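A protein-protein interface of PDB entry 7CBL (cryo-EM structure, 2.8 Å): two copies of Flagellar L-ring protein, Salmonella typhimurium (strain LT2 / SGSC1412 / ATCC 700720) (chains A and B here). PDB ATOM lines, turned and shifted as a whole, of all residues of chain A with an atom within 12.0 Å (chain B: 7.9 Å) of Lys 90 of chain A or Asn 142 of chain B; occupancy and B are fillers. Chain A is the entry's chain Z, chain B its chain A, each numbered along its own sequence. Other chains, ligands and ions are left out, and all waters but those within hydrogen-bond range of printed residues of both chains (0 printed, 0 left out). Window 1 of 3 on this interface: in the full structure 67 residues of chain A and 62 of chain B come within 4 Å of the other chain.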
ATOM      1  N   VAL A  86      -9.670 -35.341  -0.956  1.00  0.00           N
ATOM      2  CA  VAL A  86      -9.907 -33.909  -0.850  1.00  0.00           C
ATOM      3  C   VAL A  86      -9.316 -33.415   0.458  1.00  0.00           C
ATOM      4  O   VAL A  86      -9.335 -34.119   1.471  1.00  0.00           O
ATOM      5  CB  VAL A  86     -11.407 -33.572  -0.934  1.00  0.00           C
ATOM      6  CG1 VAL A  86     -11.617 -32.081  -0.922  1.00  0.00           C
ATOM      7  CG2 VAL A  86     -11.999 -34.170  -2.183  1.00  0.00           C
ATOM      8  N   SER A  87      -8.787 -32.195   0.434  1.00  0.00           N
ATOM      9  CA  SER A  87      -8.147 -31.622   1.614  1.00  0.00           C
ATOM     10  C   SER A  87      -8.158 -30.109   1.497  1.00  0.00           C
ATOM     11  O   SER A  87      -7.537 -29.560   0.587  1.00  0.00           O
ATOM     12  CB  SER A  87      -6.724 -32.138   1.751  1.00  0.00           C
ATOM     13  OG  SER A  87      -5.975 -31.315   2.621  1.00  0.00           O
ATOM     14  N   ALA A  88      -8.847 -29.438   2.415  1.00  0.00           N
ATOM     15  CA  ALA A  88      -8.921 -27.988   2.440  1.00  0.00           C
ATOM     16  C   ALA A  88      -8.537 -27.485   3.822  1.00  0.00           C
ATOM     17  O   ALA A  88      -8.649 -28.202   4.816  1.00  0.00           O
ATOM     18  CB  ALA A  88     -10.319 -27.495   2.078  1.00  0.00           C
ATOM     19  N   SER A  89      -8.100 -26.230   3.880  1.00  0.00           N
ATOM     20  CA  SER A  89      -7.633 -25.649   5.129  1.00  0.00           C
ATOM     21  C   SER A  89      -7.638 -24.134   5.018  1.00  0.00           C
ATOM     22  O   SER A  89      -7.656 -23.577   3.921  1.00  0.00           O
ATOM     23  CB  SER A  89      -6.233 -26.140   5.483  1.00  0.00           C
ATOM     24  OG  SER A  89      -5.499 -25.114   6.117  1.00  0.00           O
ATOM     25  N   LYS A  90      -7.614 -23.474   6.173  1.00  0.00           N
ATOM     26  CA  LYS A  90      -7.549 -22.022   6.232  1.00  0.00           C
ATOM     27  C   LYS A  90      -7.186 -21.610   7.649  1.00  0.00           C
ATOM     28  O   LYS A  90      -7.413 -22.355   8.604  1.00  0.00           O
ATOM     29  CB  LYS A  90      -8.866 -21.380   5.813  1.00  0.00           C
ATOM     30  CG  LYS A  90      -9.906 -21.363   6.891  1.00  0.00           C
ATOM     31  CD  LYS A  90     -11.217 -20.879   6.338  1.00  0.00           C
ATOM     32  CE  LYS A  90     -12.248 -20.728   7.423  1.00  0.00           C
ATOM     33  NZ  LYS A  90     -13.543 -20.280   6.862  1.00  0.00           N
ATOM     34  N   SER A  91      -6.629 -20.410   7.771  1.00  0.00           N
ATOM     35  CA  SER A  91      -6.223 -19.876   9.063  1.00  0.00           C
ATOM     36  C   SER A  91      -6.031 -18.375   8.929  1.00  0.00           C
ATOM     37  O   SER A  91      -5.912 -17.844   7.825  1.00  0.00           O
ATOM     38  CB  SER A  91      -4.942 -20.538   9.562  1.00  0.00           C
ATOM     39  OG  SER A  91      -3.817 -20.017   8.887  1.00  0.00           O
ATOM     40  N   SER A  92      -5.998 -17.694  10.071  1.00  0.00           N
ATOM     41  CA  SER A  92      -5.804 -16.250  10.095  1.00  0.00           C
ATOM     42  C   SER A  92      -5.502 -15.824  11.523  1.00  0.00           C
ATOM     43  O   SER A  92      -5.746 -16.567  12.477  1.00  0.00           O
ATOM     44  CB  SER A  92      -7.026 -15.511   9.555  1.00  0.00           C
ATOM     45  OG  SER A  92      -8.157 -15.743  10.367  1.00  0.00           O
ATOM     46  N   SER A  93      -4.975 -14.610  11.659  1.00  0.00           N
ATOM     47  CA  SER A  93      -4.657 -14.054  12.968  1.00  0.00           C
ATOM     48  C   SER A  93      -4.566 -12.540  12.855  1.00  0.00           C
ATOM     49  O   SER A  93      -4.663 -11.972  11.768  1.00  0.00           O
ATOM     50  CB  SER A  93      -3.356 -14.633  13.520  1.00  0.00           C
ATOM     51  OG  SER A  93      -2.255 -13.836  13.138  1.00  0.00           O
ATOM     52  N   ALA A  94      -4.380 -11.896  14.003  1.00  0.00           N
ATOM     53  CA  ALA A  94      -4.268 -10.448  14.116  1.00  0.00           C
ATOM     54  C   ALA A  94      -3.802 -10.115  15.521  1.00  0.00           C
ATOM     55  O   ALA A  94      -4.040 -10.881  16.457  1.00  0.00           O
ATOM     56  CB  ALA A  94      -5.596  -9.750  13.822  1.00  0.00           C
ATOM     57  N   GLY A 134      -5.776 -12.060  18.488  1.00  0.00           N
ATOM     58  CA  GLY A 134      -6.818 -12.960  18.054  1.00  0.00           C
ATOM     59  C   GLY A 134      -6.313 -13.839  16.929  1.00  0.00           C
ATOM     60  O   GLY A 134      -5.393 -13.480  16.203  1.00  0.00           O
ATOM     61  N   LYS A 135      -6.933 -15.006  16.794  1.00  0.00           N
ATOM     62  CA  LYS A 135      -6.510 -15.955  15.774  1.00  0.00           C
ATOM     63  C   LYS A 135      -7.594 -17.003  15.598  1.00  0.00           C
ATOM     64  O   LYS A 135      -8.509 -17.118  16.414  1.00  0.00           O
ATOM     65  CB  LYS A 135      -5.180 -16.605  16.138  1.00  0.00           C
ATOM     66  CG  LYS A 135      -5.304 -17.784  17.052  1.00  0.00           C
ATOM     67  CD  LYS A 135      -3.957 -18.137  17.629  1.00  0.00           C
ATOM     68  CE  LYS A 135      -3.905 -19.588  18.049  1.00  0.00           C
ATOM     69  NZ  LYS A 135      -4.998 -19.932  18.995  1.00  0.00           N
ATOM     70  N   GLY A 136      -7.484 -17.765  14.520  1.00  0.00           N
ATOM     71  CA  GLY A 136      -8.452 -18.811  14.249  1.00  0.00           C
ATOM     72  C   GLY A 136      -8.058 -19.581  13.012  1.00  0.00           C
ATOM     73  O   GLY A 136      -7.119 -19.218  12.297  1.00  0.00           O
ATOM     74  N   GLY A 137      -8.795 -20.656  12.765  1.00  0.00           N
ATOM     75  CA  GLY A 137      -8.527 -21.492  11.610  1.00  0.00           C
ATOM     76  C   GLY A 137      -9.519 -22.630  11.537  1.00  0.00           C
ATOM     77  O   GLY A 137     -10.371 -22.800  12.411  1.00  0.00           O
ATOM     78  N   ALA A 138      -9.393 -23.411  10.467  1.00  0.00           N
ATOM     79  CA  ALA A 138     -10.250 -24.563  10.230  1.00  0.00           C
ATOM     80  C   ALA A 138      -9.624 -25.412   9.139  1.00  0.00           C
ATOM     81  O   ALA A 138      -8.753 -24.953   8.400  1.00  0.00           O
ATOM     82  CB  ALA A 138     -11.665 -24.147   9.831  1.00  0.00           C
ATOM     83  N   ASN A 139     -10.074 -26.659   9.046  1.00  0.00           N
ATOM     84  CA  ASN A 139      -9.629 -27.533   7.970  1.00  0.00           C
ATOM     85  C   ASN A 139     -10.578 -28.711   7.859  1.00  0.00           C
ATOM     86  O   ASN A 139     -11.403 -28.956   8.738  1.00  0.00           O
ATOM     87  CB  ASN A 139      -8.194 -28.014   8.181  1.00  0.00           C
ATOM     88  CG  ASN A 139      -8.018 -28.758   9.469  1.00  0.00           C
ATOM     89  OD1 ASN A 139      -7.564 -28.196  10.460  1.00  0.00           O
ATOM     90  ND2 ASN A 139      -8.359 -30.035   9.465  1.00  0.00           N
ATOM     91  N   ALA A 140     -10.443 -29.440   6.758  1.00  0.00           N
ATOM     92  CA  ALA A 140     -11.276 -30.599   6.485  1.00  0.00           C
ATOM     93  C   ALA A 140     -10.556 -31.468   5.472  1.00  0.00           C
ATOM     94  O   ALA A 140      -9.707 -30.995   4.717  1.00  0.00           O
ATOM     95  CB  ALA A 140     -12.654 -30.194   5.968  1.00  0.00           C
ATOM     96  N   SER A 141     -10.904 -32.747   5.465  1.00  0.00           N
ATOM     97  CA  SER A 141     -10.250 -33.695   4.577  1.00  0.00           C
ATOM     98  C   SER A 141     -11.120 -34.930   4.445  1.00  0.00           C
ATOM     99  O   SER A 141     -12.019 -35.163   5.253  1.00  0.00           O
ATOM    100  CB  SER A 141      -8.867 -34.080   5.093  1.00  0.00           C
ATOM    101  OG  SER A 141      -8.672 -35.473   4.970  1.00  0.00           O
ATOM    102  N   GLN B  83      -7.021 -26.397  -6.949  1.00  0.00           N
ATOM    103  CA  GLN B  83      -5.707 -26.123  -6.372  1.00  0.00           C
ATOM    104  C   GLN B  83      -5.671 -24.633  -6.030  1.00  0.00           C
ATOM    105  O   GLN B  83      -5.282 -23.802  -6.851  1.00  0.00           O
ATOM    106  CB  GLN B  83      -4.586 -26.514  -7.320  1.00  0.00           C
ATOM    107  CG  GLN B  83      -4.841 -26.142  -8.763  1.00  0.00           C
ATOM    108  CD  GLN B  83      -3.638 -26.374  -9.641  1.00  0.00           C
ATOM    109  OE1 GLN B  83      -3.369 -25.602 -10.558  1.00  0.00           O
ATOM    110  NE2 GLN B  83      -2.906 -27.446  -9.370  1.00  0.00           N
ATOM    111  N   GLU B  84      -6.069 -24.313  -4.808  1.00  0.00           N
ATOM    112  CA  GLU B  84      -6.096 -22.944  -4.324  1.00  0.00           C
ATOM    113  C   GLU B  84      -5.030 -22.767  -3.260  1.00  0.00           C
ATOM    114  O   GLU B  84      -4.839 -23.645  -2.416  1.00  0.00           O
ATOM    115  CB  GLU B  84      -7.459 -22.588  -3.739  1.00  0.00           C
ATOM    116  CG  GLU B  84      -8.606 -22.771  -4.696  1.00  0.00           C
ATOM    117  CD  GLU B  84      -8.487 -21.887  -5.912  1.00  0.00           C
ATOM    118  OE1 GLU B  84      -8.466 -20.650  -5.753  1.00  0.00           O
ATOM    119  OE2 GLU B  84      -8.428 -22.426  -7.032  1.00  0.00           O
ATOM    120  N   ASN B  85      -4.342 -21.628  -3.302  1.00  0.00           N
ATOM    121  CA  ASN B  85      -3.290 -21.352  -2.331  1.00  0.00           C
ATOM    122  C   ASN B  85      -3.115 -19.836  -2.254  1.00  0.00           C
ATOM    123  O   ASN B  85      -2.426 -19.252  -3.091  1.00  0.00           O
ATOM    124  CB  ASN B  85      -2.001 -22.043  -2.729  1.00  0.00           C
ATOM    125  CG  ASN B  85      -0.917 -21.877  -1.702  1.00  0.00           C
ATOM    126  OD1 ASN B  85      -0.393 -20.784  -1.511  1.00  0.00           O
ATOM    127  ND2 ASN B  85      -0.562 -22.965  -1.036  1.00  0.00           N
ATOM    128  N   VAL B  86      -3.729 -19.219  -1.250  1.00  0.00           N
ATOM    129  CA  VAL B  86      -3.642 -17.779  -1.050  1.00  0.00           C
ATOM    130  C   VAL B  86      -3.002 -17.515   0.302  1.00  0.00           C
ATOM    131  O   VAL B  86      -3.216 -18.259   1.263  1.00  0.00           O
ATOM    132  CB  VAL B  86      -5.024 -17.107  -1.142  1.00  0.00           C
ATOM    133  CG1 VAL B  86      -4.895 -15.610  -1.030  1.00  0.00           C
ATOM    134  CG2 VAL B  86      -5.690 -17.476  -2.441  1.00  0.00           C
ATOM    135  N   SER B  87      -2.213 -16.447   0.374  1.00  0.00           N
ATOM    136  CA  SER B  87      -1.504 -16.110   1.603  1.00  0.00           C
ATOM    137  C   SER B  87      -1.172 -14.629   1.593  1.00  0.00           C
ATOM    138  O   SER B  87      -0.410 -14.179   0.735  1.00  0.00           O
ATOM    139  CB  SER B  87      -0.238 -16.942   1.734  1.00  0.00           C
ATOM    140  OG  SER B  87       0.644 -16.366   2.674  1.00  0.00           O
ATOM    141  N   ALA B  88      -1.725 -13.879   2.541  1.00  0.00           N
ATOM    142  CA  ALA B  88      -1.473 -12.454   2.665  1.00  0.00           C
ATOM    143  C   ALA B  88      -1.036 -12.138   4.086  1.00  0.00           C
ATOM    144  O   ALA B  88      -1.341 -12.873   5.026  1.00  0.00           O
ATOM    145  CB  ALA B  88      -2.710 -11.636   2.308  1.00  0.00           C
ATOM    146  N   ALA B 140      -3.437 -13.794   6.839  1.00  0.00           N
ATOM    147  CA  ALA B 140      -4.497 -14.715   6.468  1.00  0.00           C
ATOM    148  C   ALA B 140      -3.954 -15.658   5.412  1.00  0.00           C
ATOM    149  O   ALA B 140      -2.994 -15.342   4.710  1.00  0.00           O
ATOM    150  CB  ALA B 140      -5.730 -13.977   5.951  1.00  0.00           C
ATOM    151  N   SER B 141      -4.580 -16.824   5.309  1.00  0.00           N
ATOM    152  CA  SER B 141      -4.124 -17.836   4.370  1.00  0.00           C
ATOM    153  C   SER B 141      -5.243 -18.831   4.135  1.00  0.00           C
ATOM    154  O   SER B 141      -6.199 -18.906   4.906  1.00  0.00           O
ATOM    155  CB  SER B 141      -2.882 -18.555   4.888  1.00  0.00           C
ATOM    156  OG  SER B 141      -2.999 -19.946   4.673  1.00  0.00           O
ATOM    157  N   ASN B 142      -5.110 -19.592   3.054  1.00  0.00           N
ATOM    158  CA  ASN B 142      -6.034 -20.686   2.783  1.00  0.00           C
ATOM    159  C   ASN B 142      -5.475 -21.543   1.662  1.00  0.00           C
ATOM    160  O   ASN B 142      -4.777 -21.047   0.776  1.00  0.00           O
ATOM    161  CB  ASN B 142      -7.434 -20.175   2.424  1.00  0.00           C
ATOM    162  CG  ASN B 142      -7.638 -20.014   0.943  1.00  0.00           C
ATOM    163  OD1 ASN B 142      -7.819 -20.987   0.218  1.00  0.00           O
ATOM    164  ND2 ASN B 142      -7.632 -18.775   0.483  1.00  0.00           N
ATOM    165  N   THR B 143      -5.772 -22.837   1.726  1.00  0.00           N
ATOM    166  CA  THR B 143      -5.399 -23.793   0.696  1.00  0.00           C
ATOM    167  C   THR B 143      -6.596 -24.669   0.361  1.00  0.00           C
ATOM    168  O   THR B 143      -7.598 -24.692   1.073  1.00  0.00           O
ATOM    169  CB  THR B 143      -4.228 -24.685   1.123  1.00  0.00           C
ATOM    170  OG1 THR B 143      -4.738 -25.920   1.636  1.00  0.00           O
ATOM    171  CG2 THR B 143      -3.391 -24.015   2.193  1.00  0.00           C
ATOM    172  N   PHE B 144      -6.475 -25.390  -0.748  1.00  0.00           N
ATOM    173  CA  PHE B 144      -7.517 -26.301  -1.204  1.00  0.00           C
ATOM    174  C   PHE B 144      -6.962 -27.212  -2.284  1.00  0.00           C
ATOM    175  O   PHE B 144      -6.313 -26.736  -3.216  1.00  0.00           O
ATOM    176  CB  PHE B 144      -8.719 -25.526  -1.734  1.00  0.00           C
ATOM    177  CG  PHE B 144     -10.025 -26.236  -1.560  1.00  0.00           C
ATOM    178  CD1 PHE B 144     -10.160 -27.561  -1.912  1.00  0.00           C
ATOM    179  CD2 PHE B 144     -11.121 -25.574  -1.053  1.00  0.00           C
ATOM    180  CE1 PHE B 144     -11.360 -28.212  -1.755  1.00  0.00           C
ATOM    181  CE2 PHE B 144     -12.321 -26.222  -0.896  1.00  0.00           C
ATOM    182  CZ  PHE B 144     -12.439 -27.542  -1.248  1.00  0.00           C
ATOM    183  N   ILE B 205     -16.570 -22.054  -4.164  1.00  0.00           N
ATOM    184  CA  ILE B 205     -16.231 -23.382  -3.675  1.00  0.00           C
ATOM    185  C   ILE B 205     -16.812 -23.543  -2.281  1.00  0.00           C
ATOM    186  O   ILE B 205     -16.844 -22.596  -1.491  1.00  0.00           O
ATOM    187  CB  ILE B 205     -14.710 -23.613  -3.654  1.00  0.00           C
ATOM    188  CG1 ILE B 205     -14.062 -22.977  -4.879  1.00  0.00           C
ATOM    189  CG2 ILE B 205     -14.400 -25.084  -3.604  1.00  0.00           C
ATOM    190  CD1 ILE B 205     -12.576 -23.179  -4.941  1.00  0.00           C
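Positions printed for both chains: 86, 87, 88, 140 and 141. Of the 10 pairs that touch across the chains among the printed residues, none has its exchanged pair printed and touching as well.
The backbone NH (N) of Val 86 of chain B lies within hydrogen-bond range of the backbone carbonyl oxygen (O) of Asn 142 of chain B (2.9 Å). The backbone NH (N) of Ala 88 of chain A is in hydrogen-bond range of the backbone carbonyl oxygen (O) of Ala 140 of chain A (2.9 Å). O of Ala 138 of chain A is in hydrogen-bond range of N of Lys 90 of chain A, 2.9 Å away. The backbone carbonyl oxygen of Phe 144 of chain B sits at hydrogen-bond distance from the backbone NH of Glu 84 of chain B. O of Ala 140 of chain B lies within hydrogen-bond range of N of Ala 88 of chain B, 2.9 Å away.
Among the printed residues, pairs that only touch across the chains: Val 86 of chain A with Phe 144 of chain B (3.97 Å), Ser 87 of chain A with Phe 144 of chain B (3.7 Å), Ala 88 of chain A with Thr 143 of chain B (3.8 Å), Ala 88 of chain A with Phe 144 of chain B (3.8 Å), Ser 89 of chain A with Asn 142 of chain B (3.5 Å), Lys 90 of chain A with Ser 141 of chain B (3.6 Å), Lys 90 of chain A with Asn 142 of chain B (3.9 Å) and Ser 91 of chain A with Ala 140 of chain B (3.7 Å).
Of the 17 printed residues of chain A, 6 touch a printed residue of chain B. Hydrophobic or aromatic side chains of chain A within 4 Å of the printed part of chain B: Val 86 and Ala 88. Along chain A the printed residues that touch a printed residue of chain B span positions 86 to 91. Among the printed residues, no Asp or Glu carboxylate lies within 4 Å of a Lys or Arg side-chain nitrogen of the other chain.
The backbone NH (N) of Ser 141 of chain B lies within hydrogen-bond range of the backbone carbonyl oxygen (O) of Ser 91 of chain A, at 3.0 Å. The backbone NH (N) of Thr 143 of chain B lies within hydrogen-bond range of the backbone carbonyl oxygen (O) of Ser 89 of chain A, at 3.0 Å.
Lys 90 of chain A touches just these residues of chain B: Ser 141 and Asn 142. Ser 89 of chain A touches just these residues of chain B: Asn 142 (3.5 Å) and Thr 143 (3.0 Å). No residue of chain A comes within 4 Å of Glu 84 of chain B. No residue of chain A comes within 4 Å of Asn 85 of chain B. No residue of chain A comes within 4 Å of Ser 87 of chain B. Of chain A, only Ser 91 (3.7 Å) comes within 4 Å of Ala 140 of chain B. Of chain A, only Lys 90 (3.6 Å) and Ser 91 (3.0 Å) come within 4 Å of Ser 141 of chain B. Of chain A, only Ala 88 (3.8 Å) and Ser 89 (3.0 Å) come within 4 Å of Thr 143 of chain B. Printed residues of chain B within 4 Å of Ser 87 of chain A: Phe 144. Printed residues of chain A within 4 Å of Phe 144 of chain B: Val 86, Ser 87 and Ala 88. Printed residues of chain B within 4 Å of Ala 88 of chain A: Thr 143 and Phe 144. Printed residues of chain B within 4 Å of Val 86 of chain A: Phe 144. Of the printed residues of chain B, Ser 91 of chain A touches Ala 140 and Ser 141. The nearest printed residue of chain B that does not touch Ser 91 of chain A is Asn 142 of chain B (5.0 Å).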
